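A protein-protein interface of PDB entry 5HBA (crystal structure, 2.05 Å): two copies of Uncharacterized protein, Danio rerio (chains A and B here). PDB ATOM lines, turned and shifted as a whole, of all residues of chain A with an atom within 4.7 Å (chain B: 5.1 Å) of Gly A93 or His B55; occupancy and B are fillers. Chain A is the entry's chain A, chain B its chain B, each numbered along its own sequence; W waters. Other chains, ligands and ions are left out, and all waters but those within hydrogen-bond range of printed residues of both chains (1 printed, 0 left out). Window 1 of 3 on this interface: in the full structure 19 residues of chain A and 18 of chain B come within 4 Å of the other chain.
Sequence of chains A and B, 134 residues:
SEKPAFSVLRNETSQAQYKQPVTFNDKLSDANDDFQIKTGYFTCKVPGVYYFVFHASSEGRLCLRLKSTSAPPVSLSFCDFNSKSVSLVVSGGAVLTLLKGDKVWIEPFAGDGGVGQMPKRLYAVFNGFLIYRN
The backbone carbonyl oxygen (O) of Gly A93 is in hydrogen-bond range of the side-chain amide nitrogen (ND2) of Asn B127, at 3.3 Å.
The backbone NH (N) of Ala A94 sits at hydrogen-bond distance from the backbone carbonyl oxygen (O) of Phe A52, at 3.0 Å.
The backbone NH of Phe A54 is in hydrogen-bond range of the backbone carbonyl oxygen of Gly A92 (2.9 Å).
N of Leu A66 lies within hydrogen-bond range of O of Leu A76 (2.8 Å).
The backbone NH (N) of Asn B127 lies within hydrogen-bond range of the backbone carbonyl oxygen (O) of Val B53, at 2.8 Å.
O of His B55 sits at hydrogen-bond distance from N of Val B125 (3.0 Å).
The backbone NH (N) of Ser B57 sits at hydrogen-bond distance from the backbone carbonyl oxygen (O) of Tyr B123 (2.9 Å).
Val B53 touches Tyr A51.
Phe A78 touches His B55.
Phe A78 touches Val B89 (C to CG2, 3.9 Å).
His B55 touches Ser A91.
O of Ser A91 touches CG1 of Val B89 (3.3 Å).
Ser A91 touches Ser B91.
Gly A92 touches His B55 (CA to ND1, 3.7 Å).
N of Gly A93 touches CD2 of His B55, 3.6 Å away.
Val B125 touches Gly A93 (CG1 to O, 3.6 Å).
CA of Ala A94 touches ND2 of Asn B127, 3.6 Å away.
Printed residues of chain B within 4 Å of Gly A92: His B55 (3.7 Å).
Of the printed residues of chain B, Gly A93 touches His B55, Val B125 and Asn B127.
Printed residues of chain A within 4 Å of Val B53: Tyr A51 (3.3 Å).
Of the printed residues of chain A, His B55 touches Phe A78, Ser A91, Gly A92 and Gly A93.
Of the printed residues of chain A, Ser B91 touches Ser A91 (3.7 Å).
The nearest printed residue of chain B that does not touch Gly A93 is Val B53 (6.5 Å).
The nearest residue of chain A that does not touch His B55 is Val A53 (4.1 Å).
Of the 11 printed residues of chain A, 7 touch a printed residue of chain B.
Hydrophobic or aromatic side chains of chain A within 4 Å of the printed part of chain B: Tyr A51, Leu A76 and Phe A78.
Along chain A the printed residues that touch a printed residue of chain B span positions 51 to 94.
Hydrophobic or aromatic side chains of chain B that line the printed part of chain A: Val B53, His B55, Val B89, Tyr B123 and Val B125.
Among the printed residues, no Asp or Glu carboxylate lies within 4 Å of a Lys or Arg side-chain nitrogen of the other chain.
Ser A91 touches its own counterpart, Ser B91.
Positions printed for both chains: 53, 54 and 91.
Of the 12 pairs that touch across the chains among the printed residues, 1 has its exchanged pair printed and touching as well.
Water W1 lies within hydrogen-bond range of O of Val B89 (2.7 Å), OG of Ser B91 (2.9 Å) and N of Ser A91 (3.2 Å).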
ATOM      1  N   TYR A  51      16.064  10.207 -37.200  1.00  0.00           N
ATOM      2  CA  TYR A  51      15.411  10.500 -35.930  1.00  0.00           C
ATOM      3  C   TYR A  51      14.950  11.958 -35.894  1.00  0.00           C
ATOM      4  O   TYR A  51      15.704  12.870 -36.256  1.00  0.00           O
ATOM      5  CB  TYR A  51      16.339  10.204 -34.740  1.00  0.00           C
ATOM      6  CG  TYR A  51      15.711  10.527 -33.402  1.00  0.00           C
ATOM      7  CD1 TYR A  51      14.615   9.812 -32.943  1.00  0.00           C
ATOM      8  CD2 TYR A  51      16.200  11.562 -32.612  1.00  0.00           C
ATOM      9  CE1 TYR A  51      14.029  10.105 -31.734  1.00  0.00           C
ATOM     10  CE2 TYR A  51      15.625  11.861 -31.393  1.00  0.00           C
ATOM     11  CZ  TYR A  51      14.543  11.125 -30.961  1.00  0.00           C
ATOM     12  OH  TYR A  51      13.962  11.422 -29.760  1.00  0.00           O
ATOM     13  N   PHE A  52      13.710  12.171 -35.460  1.00  0.00           N
ATOM     14  CA  PHE A  52      13.166  13.521 -35.295  1.00  0.00           C
ATOM     15  C   PHE A  52      12.620  13.675 -33.873  1.00  0.00           C
ATOM     16  O   PHE A  52      12.052  12.732 -33.318  1.00  0.00           O
ATOM     17  CB  PHE A  52      12.022  13.766 -36.286  1.00  0.00           C
ATOM     18  CG  PHE A  52      12.453  13.812 -37.722  1.00  0.00           C
ATOM     19  CD1 PHE A  52      12.858  15.013 -38.302  1.00  0.00           C
ATOM     20  CD2 PHE A  52      12.430  12.666 -38.506  1.00  0.00           C
ATOM     21  CE1 PHE A  52      13.249  15.059 -39.644  1.00  0.00           C
ATOM     22  CE2 PHE A  52      12.818  12.707 -39.840  1.00  0.00           C
ATOM     23  CZ  PHE A  52      13.236  13.903 -40.405  1.00  0.00           C
ATOM     24  N   VAL A  53      12.781  14.861 -33.297  1.00  0.00           N
ATOM     25  CA  VAL A  53      12.250  15.138 -31.964  1.00  0.00           C
ATOM     26  C   VAL A  53      11.994  16.634 -31.831  1.00  0.00           C
ATOM     27  O   VAL A  53      12.742  17.456 -32.380  1.00  0.00           O
ATOM     28  CB  VAL A  53      13.201  14.620 -30.843  1.00  0.00           C
ATOM     29  CG1 VAL A  53      14.474  15.457 -30.763  1.00  0.00           C
ATOM     30  CG2 VAL A  53      12.499  14.609 -29.481  1.00  0.00           C
ATOM     31  N   PHE A  54      10.917  16.990 -31.138  1.00  0.00           N
ATOM     32  CA  PHE A  54      10.647  18.394 -30.861  1.00  0.00           C
ATOM     33  C   PHE A  54      10.365  18.626 -29.376  1.00  0.00           C
ATOM     34  O   PHE A  54       9.968  17.699 -28.657  1.00  0.00           O
ATOM     35  CB  PHE A  54       9.474  18.903 -31.709  1.00  0.00           C
ATOM     36  CG  PHE A  54       8.160  18.277 -31.354  1.00  0.00           C
ATOM     37  CD1 PHE A  54       7.366  18.818 -30.350  1.00  0.00           C
ATOM     38  CD2 PHE A  54       7.721  17.142 -32.014  1.00  0.00           C
ATOM     39  CE1 PHE A  54       6.168  18.239 -30.000  1.00  0.00           C
ATOM     40  CE2 PHE A  54       6.504  16.546 -31.667  1.00  0.00           C
ATOM     41  CZ  PHE A  54       5.728  17.104 -30.665  1.00  0.00           C
ATOM     42  N   LEU A  66       3.450  15.472 -35.369  1.00  0.00           N
ATOM     43  CA  LEU A  66       4.611  15.283 -36.238  1.00  0.00           C
ATOM     44  C   LEU A  66       4.090  14.655 -37.524  1.00  0.00           C
ATOM     45  O   LEU A  66       3.421  13.613 -37.482  1.00  0.00           O
ATOM     46  CB  LEU A  66       5.647  14.366 -35.582  1.00  0.00           C
ATOM     47  CG  LEU A  66       6.868  13.983 -36.420  1.00  0.00           C
ATOM     48  CD1 LEU A  66       7.833  15.193 -36.578  1.00  0.00           C
ATOM     49  CD2 LEU A  66       7.570  12.807 -35.763  1.00  0.00           C
ATOM     50  N   LEU A  76       1.589  11.723 -36.094  1.00  0.00           N
ATOM     51  CA  LEU A  76       1.631  11.367 -34.669  1.00  0.00           C
ATOM     52  C   LEU A  76       1.289  12.588 -33.825  1.00  0.00           C
ATOM     53  O   LEU A  76       1.860  13.663 -34.034  1.00  0.00           O
ATOM     54  CB  LEU A  76       3.020  10.850 -34.276  1.00  0.00           C
ATOM     55  CG  LEU A  76       3.530   9.605 -34.989  1.00  0.00           C
ATOM     56  CD1 LEU A  76       4.985   9.413 -34.654  1.00  0.00           C
ATOM     57  CD2 LEU A  76       2.708   8.369 -34.571  1.00  0.00           C
ATOM     58  N   PHE A  78       0.837  14.646 -30.090  1.00  0.00           N
ATOM     59  CA  PHE A  78       1.359  14.763 -28.739  1.00  0.00           C
ATOM     60  C   PHE A  78       0.667  15.952 -28.103  1.00  0.00           C
ATOM     61  O   PHE A  78       0.831  17.074 -28.572  1.00  0.00           O
ATOM     62  CB  PHE A  78       2.877  14.978 -28.778  1.00  0.00           C
ATOM     63  CG  PHE A  78       3.617  13.872 -29.481  1.00  0.00           C
ATOM     64  CD1 PHE A  78       3.987  12.712 -28.797  1.00  0.00           C
ATOM     65  CD2 PHE A  78       3.909  13.970 -30.832  1.00  0.00           C
ATOM     66  CE1 PHE A  78       4.654  11.673 -29.465  1.00  0.00           C
ATOM     67  CE2 PHE A  78       4.578  12.944 -31.500  1.00  0.00           C
ATOM     68  CZ  PHE A  78       4.947  11.797 -30.817  1.00  0.00           C
ATOM     69  N   SER A  91       6.911  17.196 -25.574  1.00  0.00           N
ATOM     70  CA  SER A  91       7.933  16.632 -26.444  1.00  0.00           C
ATOM     71  C   SER A  91       7.388  15.414 -27.172  1.00  0.00           C
ATOM     72  O   SER A  91       6.531  14.681 -26.648  1.00  0.00           O
ATOM     73  CB  SER A  91       9.162  16.237 -25.630  1.00  0.00           C
ATOM     74  OG  SER A  91       9.697  17.359 -24.970  1.00  0.00           O
ATOM     75  N   GLY A  92       7.880  15.195 -28.387  1.00  0.00           N
ATOM     76  CA  GLY A  92       7.435  14.071 -29.196  1.00  0.00           C
ATOM     77  C   GLY A  92       8.456  13.849 -30.288  1.00  0.00           C
ATOM     78  O   GLY A  92       9.345  14.685 -30.495  1.00  0.00           O
ATOM     79  N   GLY A  93       8.337  12.736 -30.993  1.00  0.00           N
ATOM     80  CA  GLY A  93       9.280  12.435 -32.049  1.00  0.00           C
ATOM     81  C   GLY A  93       9.220  10.985 -32.443  1.00  0.00           C
ATOM     82  O   GLY A  93       8.482  10.191 -31.832  1.00  0.00           O
ATOM     83  N   ALA A  94       9.986  10.626 -33.470  1.00  0.00           N
ATOM     84  CA  ALA A  94       9.913   9.278 -34.024  1.00  0.00           C
ATOM     85  C   ALA A  94      11.134   8.942 -34.858  1.00  0.00           C
ATOM     86  O   ALA A  94      11.852   9.836 -35.307  1.00  0.00           O
ATOM     87  CB  ALA A  94       8.643   9.113 -34.861  1.00  0.00           C
ATOM     88  N   VAL B  53      14.248   6.147 -26.430  1.00  0.00           N
ATOM     89  CA  VAL B  53      13.427   7.281 -25.987  1.00  0.00           C
ATOM     90  C   VAL B  53      11.943   6.992 -26.203  1.00  0.00           C
ATOM     91  O   VAL B  53      11.565   6.404 -27.215  1.00  0.00           O
ATOM     92  CB  VAL B  53      13.855   8.627 -26.657  1.00  0.00           C
ATOM     93  CG1 VAL B  53      13.612   8.591 -28.173  1.00  0.00           C
ATOM     94  CG2 VAL B  53      13.094   9.796 -26.041  1.00  0.00           C
ATOM     95  N   PHE B  54      11.104   7.356 -25.233  1.00  0.00           N
ATOM     96  CA  PHE B  54       9.664   7.192 -25.427  1.00  0.00           C
ATOM     97  C   PHE B  54       8.926   8.496 -25.171  1.00  0.00           C
ATOM     98  O   PHE B  54       9.398   9.379 -24.434  1.00  0.00           O
ATOM     99  CB  PHE B  54       9.092   6.088 -24.518  1.00  0.00           C
ATOM    100  CG  PHE B  54       9.209   6.406 -23.056  1.00  0.00           C
ATOM    101  CD1 PHE B  54       8.210   7.119 -22.403  1.00  0.00           C
ATOM    102  CD2 PHE B  54      10.336   6.023 -22.339  1.00  0.00           C
ATOM    103  CE1 PHE B  54       8.336   7.452 -21.044  1.00  0.00           C
ATOM    104  CE2 PHE B  54      10.465   6.340 -20.992  1.00  0.00           C
ATOM    105  CZ  PHE B  54       9.463   7.056 -20.345  1.00  0.00           C
ATOM    106  N   HIS B  55       7.751   8.609 -25.772  1.00  0.00           N
ATOM    107  CA  HIS B  55       6.855   9.712 -25.474  1.00  0.00           C
ATOM    108  C   HIS B  55       5.483   9.102 -25.290  1.00  0.00           C
ATOM    109  O   HIS B  55       5.008   8.378 -26.169  1.00  0.00           O
ATOM    110  CB  HIS B  55       6.840  10.704 -26.638  1.00  0.00           C
ATOM    111  CG  HIS B  55       8.205  11.069 -27.141  1.00  0.00           C
ATOM    112  ND1 HIS B  55       8.978  12.053 -26.566  1.00  0.00           N
ATOM    113  CD2 HIS B  55       8.927  10.592 -28.190  1.00  0.00           C
ATOM    114  CE1 HIS B  55      10.117  12.163 -27.223  1.00  0.00           C
ATOM    115  NE2 HIS B  55      10.111  11.292 -28.216  1.00  0.00           N
ATOM    116  N   ALA B  56       4.843   9.348 -24.151  1.00  0.00           N
ATOM    117  CA  ALA B  56       3.557   8.692 -23.901  1.00  0.00           C
ATOM    118  C   ALA B  56       2.580   9.564 -23.132  1.00  0.00           C
ATOM    119  O   ALA B  56       2.983  10.474 -22.404  1.00  0.00           O
ATOM    120  CB  ALA B  56       3.748   7.353 -23.181  1.00  0.00           C
ATOM    121  N   SER B  57       1.292   9.275 -23.300  1.00  0.00           N
ATOM    122  CA  SER B  57       0.267  10.026 -22.593  1.00  0.00           C
ATOM    123  C   SER B  57      -0.858   9.125 -22.121  1.00  0.00           C
ATOM    124  O   SER B  57      -1.217   8.136 -22.768  1.00  0.00           O
ATOM    125  CB  SER B  57      -0.276  11.193 -23.435  1.00  0.00           C
ATOM    126  OG  SER B  57      -0.802  10.756 -24.678  1.00  0.00           O
ATOM    127  N   VAL B  89       1.897  14.531 -21.928  1.00  0.00           N
ATOM    128  CA  VAL B  89       2.902  13.660 -22.538  1.00  0.00           C
ATOM    129  C   VAL B  89       4.145  13.571 -21.658  1.00  0.00           C
ATOM    130  O   VAL B  89       4.833  14.572 -21.457  1.00  0.00           O
ATOM    131  CB  VAL B  89       3.336  14.174 -23.932  1.00  0.00           C
ATOM    132  CG1 VAL B  89       4.409  13.250 -24.532  1.00  0.00           C
ATOM    133  CG2 VAL B  89       2.123  14.297 -24.881  1.00  0.00           C
ATOM    134  N   VAL B  90       4.428  12.381 -21.128  1.00  0.00           N
ATOM    135  CA  VAL B  90       5.691  12.138 -20.431  1.00  0.00           C
ATOM    136  C   VAL B  90       6.723  11.580 -21.415  1.00  0.00           C
ATOM    137  O   VAL B  90       6.391  10.785 -22.311  1.00  0.00           O
ATOM    138  CB  VAL B  90       5.515  11.182 -19.211  1.00  0.00           C
ATOM    139  CG1 VAL B  90       5.049   9.832 -19.654  1.00  0.00           C
ATOM    140  CG2 VAL B  90       6.816  11.034 -18.441  1.00  0.00           C
ATOM    141  N   SER B  91       7.969  12.018 -21.276  1.00  0.00           N
ATOM    142  CA  SER B  91       9.033  11.518 -22.127  1.00  0.00           C
ATOM    143  C   SER B  91      10.194  11.054 -21.267  1.00  0.00           C
ATOM    144  O   SER B  91      10.393  11.557 -20.153  1.00  0.00           O
ATOM    145  CB  SER B  91       9.496  12.603 -23.106  1.00  0.00           C
ATOM    146  OG  SER B  91       8.447  12.982 -23.987  1.00  0.00           O
ATOM    147  N   TYR B 123      -1.307   5.943 -24.882  1.00  0.00           N
ATOM    148  CA  TYR B 123      -0.799   6.267 -26.211  1.00  0.00           C
ATOM    149  C   TYR B 123       0.710   6.352 -26.034  1.00  0.00           C
ATOM    150  O   TYR B 123       1.187   7.056 -25.150  1.00  0.00           O
ATOM    151  CB  TYR B 123      -1.368   7.612 -26.672  1.00  0.00           C
ATOM    152  CG  TYR B 123      -0.909   8.095 -28.039  1.00  0.00           C
ATOM    153  CD1 TYR B 123      -1.582   7.717 -29.197  1.00  0.00           C
ATOM    154  CD2 TYR B 123       0.175   8.961 -28.165  1.00  0.00           C
ATOM    155  CE1 TYR B 123      -1.175   8.178 -30.453  1.00  0.00           C
ATOM    156  CE2 TYR B 123       0.587   9.422 -29.411  1.00  0.00           C
ATOM    157  CZ  TYR B 123      -0.090   9.025 -30.547  1.00  0.00           C
ATOM    158  OH  TYR B 123       0.309   9.478 -31.793  1.00  0.00           O
ATOM    159  N   ALA B 124       1.463   5.607 -26.832  1.00  0.00           N
ATOM    160  CA  ALA B 124       2.912   5.592 -26.661  1.00  0.00           C
ATOM    161  C   ALA B 124       3.664   5.418 -27.975  1.00  0.00           C
ATOM    162  O   ALA B 124       3.257   4.632 -28.843  1.00  0.00           O
ATOM    163  CB  ALA B 124       3.317   4.498 -25.681  1.00  0.00           C
ATOM    164  N   VAL B 125       4.769   6.152 -28.103  1.00  0.00           N
ATOM    165  CA  VAL B 125       5.706   5.954 -29.197  1.00  0.00           C
ATOM    166  C   VAL B 125       7.039   5.621 -28.558  1.00  0.00           C
ATOM    167  O   VAL B 125       7.531   6.361 -27.704  1.00  0.00           O
ATOM    168  CB  VAL B 125       5.871   7.223 -30.062  1.00  0.00           C
ATOM    169  CG1 VAL B 125       6.893   6.983 -31.171  1.00  0.00           C
ATOM    170  CG2 VAL B 125       4.526   7.646 -30.662  1.00  0.00           C
ATOM    171  N   ASN B 127      11.024   4.596 -29.330  1.00  0.00           N
ATOM    172  CA  ASN B 127      12.051   4.698 -30.369  1.00  0.00           C
ATOM    173  C   ASN B 127      13.398   4.228 -29.845  1.00  0.00           C
ATOM    174  O   ASN B 127      13.710   4.398 -28.658  1.00  0.00           O
ATOM    175  CB  ASN B 127      12.229   6.166 -30.786  1.00  0.00           C
ATOM    176  CG  ASN B 127      10.931   6.817 -31.250  1.00  0.00           C
ATOM    177  OD1 ASN B 127      10.181   6.243 -32.046  1.00  0.00           O
ATOM    178  ND2 ASN B 127      10.675   8.033 -30.771  1.00  0.00           N
HETATM  179  O   HOH W   1       6.859  15.283 -23.059  1.00  0.00           O
